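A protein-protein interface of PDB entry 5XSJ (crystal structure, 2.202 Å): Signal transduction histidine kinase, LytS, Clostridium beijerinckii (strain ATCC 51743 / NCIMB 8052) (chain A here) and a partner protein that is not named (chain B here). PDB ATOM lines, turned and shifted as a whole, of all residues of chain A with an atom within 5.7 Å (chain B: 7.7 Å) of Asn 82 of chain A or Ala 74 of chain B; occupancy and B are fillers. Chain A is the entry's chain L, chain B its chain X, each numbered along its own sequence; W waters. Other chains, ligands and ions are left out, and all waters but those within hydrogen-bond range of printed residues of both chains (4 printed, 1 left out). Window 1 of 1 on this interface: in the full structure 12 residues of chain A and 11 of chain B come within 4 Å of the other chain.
Water W4 lies within hydrogen-bond range of OD2 of Asp 85 of chain A (2.5 Å), NZ of Lys 75 of chain B (2.7 Å) and OD1 of Asn 82 of chain A (3.0 Å). Water W1 lies within hydrogen-bond range of O of Met 70 of chain B (2.7 Å), OG1 of Thr 83 of chain A (2.9 Å) and OH of Tyr 124 of chain A (2.9 Å). Water W3 lies within hydrogen-bond range of the side-chain amino group (NZ) of Lys 75 of chain B and the backbone carbonyl oxygen (O) of Asp 85 of chain A. Water W2 lies within hydrogen-bond range of the backbone carbonyl oxygen of Lys 75 of chain B and the guanidinium group of Arg 78 of chain A.
Of the printed residues of chain A, Ala 74 of chain B touches Asn 82 (3.2 Å), Thr 83 (3.3 Å) and Tyr 124 (3.9 Å). Printed residues of chain B within 4 Å of Tyr 124 of chain A: Ala 74 (3.9 Å). Of the printed residues of chain B, Thr 83 of chain A touches Ser 73 (3.3 Å) and Ala 74 (3.3 Å). Of the printed residues of chain B, Asp 79 of chain A touches Lys 20. Printed residues of chain A within 4 Å of Lys 20 of chain B: Arg 78 (3.6 Å) and Asp 79 (2.6 Å). Of the printed residues of chain A, Lys 75 of chain B touches Asn 82, Asp 85 and Ser 86. The nearest printed residue of chain B that does not touch Thr 83 of chain A is Met 70 of chain B (4.9 Å).
Of the 12 printed residues of chain A, 7 touch a printed residue of chain B. Printed residues of chain A that touch a printed residue of chain B: Arg 78, Asp 79, Asn 82, Thr 83, Asp 85, Ser 86 and Tyr 124. Among the printed residues, 11 pairs touch across the chains. Among the printed residues, Asp or Glu carboxylates within 4 Å of a Lys or Arg side-chain nitrogen of the other chain: Asp 79 of chain A with Lys 20 of chain B (2.6 Å).
The side-chain amino group of Lys 20 of chain B is in salt-bridge range of the side-chain carboxylate of Glu 52 of chain B (2.6 Å). The backbone carbonyl oxygen (O) of Lys 20 of chain B is in hydrogen-bond range of the backbone NH (N) of Ser 77 of chain B (3.1 Å). The side-chain hydroxyl of Ser 73 of chain B is in hydrogen-bond range of the backbone carbonyl oxygen of Asp 69 of chain B, at 2.9 Å. O of Arg 78 of chain A sits at hydrogen-bond distance from ND2 of Asn 82 of chain A, at 3.3 Å. The side-chain hydroxyl (OG1) of Thr 83 of chain A is in hydrogen-bond range of the backbone carbonyl oxygen (O) of Asp 79 of chain A. The side-chain hydroxyl (OG) of Ser 86 of chain A lies within hydrogen-bond range of the backbone carbonyl oxygen (O) of Asn 82 of chain A (3.5 Å).
Arg 78 of chain A touches Lys 20 of chain B. Lys 75 of chain B touches Asn 82 of chain A (CE to O, 3.8 Å). Ser 73 of chain B touches Thr 83 of chain A (O to CA, 3.3 Å). Ala 74 of chain B touches Thr 83 of chain A. Asp 85 of chain A touches Lys 75 of chain B (CB to NZ, 3.7 Å). Ser 86 of chain A touches Lys 75 of chain B. OH of Tyr 124 of chain A touches CB of Ala 74 of chain B, 3.9 Å away.
The side-chain carboxylate of Asp 79 of chain A lies within salt-bridge range of the side-chain amino group of Lys 20 of chain B. The side-chain hydroxyl (OG) of Ser 86 of chain A sits at hydrogen-bond distance from the backbone carbonyl oxygen (O) of Ser 73 of chain B, at 2.7 Å. ND2 of Asn 82 of chain A sits close to O of Ala 74 of chain B (3.4 Å). O of Ser 73 of chain B lies close to O of Asn 82 of chain A (3.3 Å).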
ATOM      1  N   LEU A  77     -14.631  31.877 -26.948  1.00  0.00           N
ATOM      2  CA  LEU A  77     -14.657  32.057 -25.501  1.00  0.00           C
ATOM      3  C   LEU A  77     -16.075  32.321 -25.035  1.00  0.00           C
ATOM      4  O   LEU A  77     -16.502  31.804 -23.996  1.00  0.00           O
ATOM      5  CB  LEU A  77     -13.735  33.198 -25.068  1.00  0.00           C
ATOM      6  CG  LEU A  77     -12.265  32.823 -24.915  1.00  0.00           C
ATOM      7  CD1 LEU A  77     -11.390  34.057 -24.789  1.00  0.00           C
ATOM      8  CD2 LEU A  77     -12.097  31.931 -23.714  1.00  0.00           C
ATOM      9  N   ARG A  78     -16.806  33.117 -25.809  1.00  0.00           N
ATOM     10  CA  ARG A  78     -18.208  33.355 -25.505  1.00  0.00           C
ATOM     11  C   ARG A  78     -19.008  32.044 -25.562  1.00  0.00           C
ATOM     12  O   ARG A  78     -19.817  31.777 -24.689  1.00  0.00           O
ATOM     13  CB  ARG A  78     -18.817  34.390 -26.458  1.00  0.00           C
ATOM     14  CG  ARG A  78     -20.309  34.612 -26.210  1.00  0.00           C
ATOM     15  CD  ARG A  78     -20.886  35.710 -27.077  1.00  0.00           C
ATOM     16  NE  ARG A  78     -20.808  35.380 -28.495  1.00  0.00           N
ATOM     17  CZ  ARG A  78     -21.200  36.197 -29.469  1.00  0.00           C
ATOM     18  NH1 ARG A  78     -21.694  37.399 -29.171  1.00  0.00           N
ATOM     19  NH2 ARG A  78     -21.092  35.815 -30.738  1.00  0.00           N
ATOM     20  N   ASP A  79     -18.779  31.226 -26.588  1.00  0.00           N
ATOM     21  CA  ASP A  79     -19.469  29.939 -26.677  1.00  0.00           C
ATOM     22  C   ASP A  79     -19.116  29.042 -25.492  1.00  0.00           C
ATOM     23  O   ASP A  79     -19.964  28.346 -24.944  1.00  0.00           O
ATOM     24  CB  ASP A  79     -19.119  29.213 -27.982  1.00  0.00           C
ATOM     25  CG  ASP A  79     -19.769  29.843 -29.206  1.00  0.00           C
ATOM     26  OD1 ASP A  79     -20.739  30.624 -29.050  1.00  0.00           O
ATOM     27  OD2 ASP A  79     -19.308  29.539 -30.334  1.00  0.00           O
ATOM     28  N   LEU A  80     -17.842  29.043 -25.125  1.00  0.00           N
ATOM     29  CA  LEU A  80     -17.374  28.200 -24.043  1.00  0.00           C
ATOM     30  C   LEU A  80     -17.944  28.688 -22.698  1.00  0.00           C
ATOM     31  O   LEU A  80     -18.408  27.898 -21.886  1.00  0.00           O
ATOM     32  CB  LEU A  80     -15.841  28.179 -24.032  1.00  0.00           C
ATOM     33  CG  LEU A  80     -15.175  27.594 -22.785  1.00  0.00           C
ATOM     34  CD1 LEU A  80     -15.609  26.142 -22.526  1.00  0.00           C
ATOM     35  CD2 LEU A  80     -13.666  27.711 -22.891  1.00  0.00           C
ATOM     36  N   ASP A  81     -17.923  29.995 -22.483  1.00  0.00           N
ATOM     37  CA  ASP A  81     -18.445  30.594 -21.250  1.00  0.00           C
ATOM     38  C   ASP A  81     -19.932  30.308 -21.070  1.00  0.00           C
ATOM     39  O   ASP A  81     -20.380  29.890 -20.000  1.00  0.00           O
ATOM     40  CB  ASP A  81     -18.193  32.102 -21.268  1.00  0.00           C
ATOM     41  CG  ASP A  81     -18.347  32.749 -19.886  1.00  0.00           C
ATOM     42  OD1 ASP A  81     -18.193  32.052 -18.855  1.00  0.00           O
ATOM     43  OD2 ASP A  81     -18.620  33.967 -19.839  1.00  0.00           O
ATOM     44  N   ASN A  82     -20.706  30.532 -22.126  1.00  0.00           N
ATOM     45  CA  ASN A  82     -22.124  30.198 -22.093  1.00  0.00           C
ATOM     46  C   ASN A  82     -22.389  28.712 -21.920  1.00  0.00           C
ATOM     47  O   ASN A  82     -23.296  28.318 -21.213  1.00  0.00           O
ATOM     48  CB  ASN A  82     -22.797  30.700 -23.356  1.00  0.00           C
ATOM     49  CG  ASN A  82     -23.014  32.175 -23.316  1.00  0.00           C
ATOM     50  OD1 ASN A  82     -23.267  32.730 -22.245  1.00  0.00           O
ATOM     51  ND2 ASN A  82     -22.896  32.834 -24.460  1.00  0.00           N
ATOM     52  N   THR A  83     -21.579  27.881 -22.556  1.00  0.00           N
ATOM     53  CA  THR A  83     -21.776  26.444 -22.465  1.00  0.00           C
ATOM     54  C   THR A  83     -21.480  25.975 -21.042  1.00  0.00           C
ATOM     55  O   THR A  83     -22.161  25.096 -20.517  1.00  0.00           O
ATOM     56  CB  THR A  83     -20.889  25.701 -23.498  1.00  0.00           C
ATOM     57  OG1 THR A  83     -21.192  26.202 -24.803  1.00  0.00           O
ATOM     58  CG2 THR A  83     -21.122  24.206 -23.474  1.00  0.00           C
ATOM     59  N   LEU A  84     -20.475  26.569 -20.404  1.00  0.00           N
ATOM     60  CA  LEU A  84     -20.205  26.247 -19.004  1.00  0.00           C
ATOM     61  C   LEU A  84     -21.389  26.623 -18.122  1.00  0.00           C
ATOM     62  O   LEU A  84     -21.774  25.852 -17.239  1.00  0.00           O
ATOM     63  CB  LEU A  84     -18.941  26.952 -18.503  1.00  0.00           C
ATOM     64  CG  LEU A  84     -18.522  26.480 -17.097  1.00  0.00           C
ATOM     65  CD1 LEU A  84     -18.037  25.035 -17.145  1.00  0.00           C
ATOM     66  CD2 LEU A  84     -17.451  27.374 -16.482  1.00  0.00           C
ATOM     67  N   ASP A  85     -21.981  27.795 -18.357  1.00  0.00           N
ATOM     68  CA  ASP A  85     -23.170  28.189 -17.602  1.00  0.00           C
ATOM     69  C   ASP A  85     -24.282  27.143 -17.765  1.00  0.00           C
ATOM     70  O   ASP A  85     -25.014  26.866 -16.807  1.00  0.00           O
ATOM     71  CB  ASP A  85     -23.692  29.565 -18.040  1.00  0.00           C
ATOM     72  CG  ASP A  85     -22.763  30.717 -17.649  1.00  0.00           C
ATOM     73  OD1 ASP A  85     -21.904  30.555 -16.755  1.00  0.00           O
ATOM     74  OD2 ASP A  85     -22.905  31.803 -18.247  1.00  0.00           O
ATOM     75  N   SER A  86     -24.409  26.566 -18.966  1.00  0.00           N
ATOM     76  CA  SER A  86     -25.424  25.527 -19.197  1.00  0.00           C
ATOM     77  C   SER A  86     -25.124  24.268 -18.399  1.00  0.00           C
ATOM     78  O   SER A  86     -26.013  23.619 -17.874  1.00  0.00           O
ATOM     79  CB  SER A  86     -25.525  25.164 -20.683  1.00  0.00           C
ATOM     80  OG  SER A  86     -26.051  26.232 -21.446  1.00  0.00           O
ATOM     81  N   TYR A  87     -23.856  23.907 -18.350  1.00  0.00           N
ATOM     82  CA  TYR A  87     -23.415  22.796 -17.527  1.00  0.00           C
ATOM     83  C   TYR A  87     -23.710  23.054 -16.061  1.00  0.00           C
ATOM     84  O   TYR A  87     -24.170  22.176 -15.344  1.00  0.00           O
ATOM     85  CB  TYR A  87     -21.921  22.576 -17.719  1.00  0.00           C
ATOM     86  CG  TYR A  87     -21.311  21.727 -16.643  1.00  0.00           C
ATOM     87  CD1 TYR A  87     -21.522  20.355 -16.625  1.00  0.00           C
ATOM     88  CD2 TYR A  87     -20.504  22.286 -15.647  1.00  0.00           C
ATOM     89  CE1 TYR A  87     -20.955  19.544 -15.641  1.00  0.00           C
ATOM     90  CE2 TYR A  87     -19.934  21.479 -14.650  1.00  0.00           C
ATOM     91  CZ  TYR A  87     -20.156  20.105 -14.656  1.00  0.00           C
ATOM     92  OH  TYR A  87     -19.596  19.287 -13.677  1.00  0.00           O
ATOM     93  N   TYR A 124     -14.393  23.001 -27.061  1.00  0.00           N
ATOM     94  CA  TYR A 124     -14.057  24.426 -27.166  1.00  0.00           C
ATOM     95  C   TYR A 124     -12.638  24.669 -26.637  1.00  0.00           C
ATOM     96  O   TYR A 124     -11.860  25.418 -27.219  1.00  0.00           O
ATOM     97  CB  TYR A 124     -15.066  25.297 -26.406  1.00  0.00           C
ATOM     98  CG  TYR A 124     -16.448  25.273 -27.016  1.00  0.00           C
ATOM     99  CD1 TYR A 124     -16.629  25.496 -28.376  1.00  0.00           C
ATOM    100  CD2 TYR A 124     -17.564  24.991 -26.249  1.00  0.00           C
ATOM    101  CE1 TYR A 124     -17.882  25.460 -28.948  1.00  0.00           C
ATOM    102  CE2 TYR A 124     -18.833  24.953 -26.815  1.00  0.00           C
ATOM    103  CZ  TYR A 124     -18.983  25.189 -28.162  1.00  0.00           C
ATOM    104  OH  TYR A 124     -20.230  25.140 -28.739  1.00  0.00           O
ATOM    105  N   LYS B  20     -24.013  35.691 -33.131  1.00  0.00           N
ATOM    106  CA  LYS B  20     -23.686  34.527 -33.935  1.00  0.00           C
ATOM    107  C   LYS B  20     -24.924  33.696 -34.201  1.00  0.00           C
ATOM    108  O   LYS B  20     -25.629  33.283 -33.282  1.00  0.00           O
ATOM    109  CB  LYS B  20     -22.625  33.668 -33.259  1.00  0.00           C
ATOM    110  CG  LYS B  20     -22.492  32.317 -33.924  1.00  0.00           C
ATOM    111  CD  LYS B  20     -21.071  31.841 -33.892  1.00  0.00           C
ATOM    112  CE  LYS B  20     -20.827  31.035 -32.661  1.00  0.00           C
ATOM    113  NZ  LYS B  20     -19.463  30.454 -32.795  1.00  0.00           N
ATOM    114  N   VAL B  22     -26.418  30.245 -35.850  1.00  0.00           N
ATOM    115  CA  VAL B  22     -26.043  28.899 -36.259  1.00  0.00           C
ATOM    116  C   VAL B  22     -26.993  28.396 -37.341  1.00  0.00           C
ATOM    117  O   VAL B  22     -28.214  28.496 -37.202  1.00  0.00           O
ATOM    118  CB  VAL B  22     -26.041  27.934 -35.063  1.00  0.00           C
ATOM    119  CG1 VAL B  22     -25.896  26.505 -35.520  1.00  0.00           C
ATOM    120  CG2 VAL B  22     -24.904  28.321 -34.074  1.00  0.00           C
ATOM    121  N   GLU B  52     -22.482  30.701 -38.408  1.00  0.00           N
ATOM    122  CA  GLU B  52     -21.715  29.467 -38.267  1.00  0.00           C
ATOM    123  C   GLU B  52     -22.490  28.348 -38.950  1.00  0.00           C
ATOM    124  O   GLU B  52     -23.620  28.032 -38.565  1.00  0.00           O
ATOM    125  CB  GLU B  52     -21.444  29.136 -36.795  1.00  0.00           C
ATOM    126  CG  GLU B  52     -20.812  27.761 -36.515  1.00  0.00           C
ATOM    127  CD  GLU B  52     -20.499  27.570 -35.020  1.00  0.00           C
ATOM    128  OE1 GLU B  52     -20.266  28.576 -34.339  1.00  0.00           O
ATOM    129  OE2 GLU B  52     -20.509  26.432 -34.509  1.00  0.00           O
ATOM    130  N   PHE B  68     -27.670  20.866 -32.823  1.00  0.00           N
ATOM    131  CA  PHE B  68     -28.684  21.787 -32.334  1.00  0.00           C
ATOM    132  C   PHE B  68     -28.542  21.922 -30.818  1.00  0.00           C
ATOM    133  O   PHE B  68     -28.674  23.011 -30.255  1.00  0.00           O
ATOM    134  CB  PHE B  68     -30.086  21.293 -32.724  1.00  0.00           C
ATOM    135  CG  PHE B  68     -31.187  22.316 -32.506  1.00  0.00           C
ATOM    136  CD1 PHE B  68     -31.678  22.575 -31.229  1.00  0.00           C
ATOM    137  CD2 PHE B  68     -31.750  22.990 -33.580  1.00  0.00           C
ATOM    138  CE1 PHE B  68     -32.695  23.508 -31.024  1.00  0.00           C
ATOM    139  CE2 PHE B  68     -32.765  23.920 -33.385  1.00  0.00           C
ATOM    140  CZ  PHE B  68     -33.236  24.185 -32.102  1.00  0.00           C
ATOM    141  N   ASP B  69     -28.265  20.802 -30.165  1.00  0.00           N
ATOM    142  CA  ASP B  69     -28.020  20.803 -28.730  1.00  0.00           C
ATOM    143  C   ASP B  69     -26.781  21.636 -28.344  1.00  0.00           C
ATOM    144  O   ASP B  69     -26.812  22.358 -27.345  1.00  0.00           O
ATOM    145  CB  ASP B  69     -27.870  19.369 -28.233  1.00  0.00           C
ATOM    146  CG  ASP B  69     -27.953  19.268 -26.734  1.00  0.00           C
ATOM    147  OD1 ASP B  69     -26.925  18.932 -26.095  1.00  0.00           O
ATOM    148  OD2 ASP B  69     -29.051  19.538 -26.196  1.00  0.00           O
ATOM    149  N   MET B  70     -25.704  21.537 -29.132  1.00  0.00           N
ATOM    150  CA  MET B  70     -24.488  22.323 -28.890  1.00  0.00           C
ATOM    151  C   MET B  70     -24.773  23.823 -28.985  1.00  0.00           C
ATOM    152  O   MET B  70     -24.336  24.602 -28.133  1.00  0.00           O
ATOM    153  CB  MET B  70     -23.360  21.946 -29.878  1.00  0.00           C
ATOM    154  CG  MET B  70     -22.880  20.480 -29.777  1.00  0.00           C
ATOM    155  SD  MET B  70     -21.549  20.011 -30.938  1.00  0.00           S
ATOM    156  CE  MET B  70     -20.489  21.431 -30.686  1.00  0.00           C
ATOM    157  N   ALA B  71     -25.495  24.231 -30.021  1.00  0.00           N
ATOM    158  CA  ALA B  71     -25.863  25.640 -30.184  1.00  0.00           C
ATOM    159  C   ALA B  71     -26.768  26.116 -29.042  1.00  0.00           C
ATOM    160  O   ALA B  71     -26.644  27.238 -28.549  1.00  0.00           O
ATOM    161  CB  ALA B  71     -26.554  25.864 -31.551  1.00  0.00           C
ATOM    162  N   THR B  72     -27.691  25.270 -28.617  1.00  0.00           N
ATOM    163  CA  THR B  72     -28.547  25.637 -27.500  1.00  0.00           C
ATOM    164  C   THR B  72     -27.695  25.878 -26.254  1.00  0.00           C
ATOM    165  O   THR B  72     -27.807  26.915 -25.632  1.00  0.00           O
ATOM    166  CB  THR B  72     -29.594  24.562 -27.237  1.00  0.00           C
ATOM    167  OG1 THR B  72     -30.449  24.469 -28.390  1.00  0.00           O
ATOM    168  CG2 THR B  72     -30.425  24.910 -25.998  1.00  0.00           C
ATOM    169  N   SER B  73     -26.794  24.948 -25.950  1.00  0.00           N
ATOM    170  CA  SER B  73     -25.928  25.055 -24.785  1.00  0.00           C
ATOM    171  C   SER B  73     -25.050  26.300 -24.817  1.00  0.00           C
ATOM    172  O   SER B  73     -24.793  26.932 -23.782  1.00  0.00           O
ATOM    173  CB  SER B  73     -25.055  23.817 -24.686  1.00  0.00           C
ATOM    174  OG  SER B  73     -25.876  22.676 -24.586  1.00  0.00           O
ATOM    175  N   ALA B  74     -24.615  26.661 -26.016  1.00  0.00           N
ATOM    176  CA  ALA B  74     -23.743  27.805 -26.219  1.00  0.00           C
ATOM    177  C   ALA B  74     -24.543  29.119 -26.215  1.00  0.00           C
ATOM    178  O   ALA B  74     -23.974  30.216 -26.308  1.00  0.00           O
ATOM    179  CB  ALA B  74     -22.946  27.636 -27.555  1.00  0.00           C
ATOM    180  N   LYS B  75     -25.861  28.993 -26.110  1.00  0.00           N
ATOM    181  CA  LYS B  75     -26.756  30.146 -26.070  1.00  0.00           C
ATOM    182  C   LYS B  75     -26.422  31.128 -27.178  1.00  0.00           C
ATOM    183  O   LYS B  75     -26.195  32.307 -26.919  1.00  0.00           O
ATOM    184  CB  LYS B  75     -26.680  30.851 -24.710  1.00  0.00           C
ATOM    185  CG  LYS B  75     -26.848  29.917 -23.519  1.00  0.00           C
ATOM    186  CD  LYS B  75     -26.739  30.688 -22.208  1.00  0.00           C
ATOM    187  CE  LYS B  75     -26.765  29.756 -21.001  1.00  0.00           C
ATOM    188  NZ  LYS B  75     -26.824  30.547 -19.736  1.00  0.00           N
ATOM    189  N   VAL B  76     -26.346  30.632 -28.410  1.00  0.00           N
ATOM    190  CA  VAL B  76     -26.098  31.497 -29.560  1.00  0.00           C
ATOM    191  C   VAL B  76     -27.282  32.448 -29.749  1.00  0.00           C
ATOM    192  O   VAL B  76     -28.351  32.246 -29.169  1.00  0.00           O
ATOM    193  CB  VAL B  76     -25.871  30.675 -30.847  1.00  0.00           C
ATOM    194  CG1 VAL B  76     -24.602  29.828 -30.721  1.00  0.00           C
ATOM    195  CG2 VAL B  76     -27.099  29.800 -31.152  1.00  0.00           C
ATOM    196  N   SER B  77     -27.099  33.475 -30.566  1.00  0.00           N
ATOM    197  CA  SER B  77     -28.139  34.478 -30.762  1.00  0.00           C
ATOM    198  C   SER B  77     -29.317  33.986 -31.597  1.00  0.00           C
ATOM    199  O   SER B  77     -30.399  34.564 -31.543  1.00  0.00           O
ATOM    200  CB  SER B  77     -27.535  35.718 -31.412  1.00  0.00           C
ATOM    201  OG  SER B  77     -26.212  35.910 -30.949  1.00  0.00           O
ATOM    202  N   ILE B 101     -33.675  31.574 -27.186  1.00  0.00           N
ATOM    203  CA  ILE B 101     -32.990  31.523 -28.478  1.00  0.00           C
ATOM    204  C   ILE B 101     -34.013  31.477 -29.609  1.00  0.00           C
ATOM    205  O   ILE B 101     -34.782  30.533 -29.704  1.00  0.00           O
ATOM    206  CB  ILE B 101     -32.057  30.308 -28.577  1.00  0.00           C
ATOM    207  CG1 ILE B 101     -31.106  30.280 -27.371  1.00  0.00           C
ATOM    208  CG2 ILE B 101     -31.295  30.335 -29.914  1.00  0.00           C
ATOM    209  CD1 ILE B 101     -30.351  28.997 -27.246  1.00  0.00           C
HETATM  210  O   HOH W   1     -22.096  24.186 -26.694  1.00  0.00           O
HETATM  211  O   HOH W   2     -24.008  34.141 -28.193  1.00  0.00           O
HETATM  212  O   HOH W   3     -27.594  28.689 -17.843  1.00  0.00           O
HETATM  213  O   HOH W   4     -24.894  32.441 -19.687  1.00  0.00           O
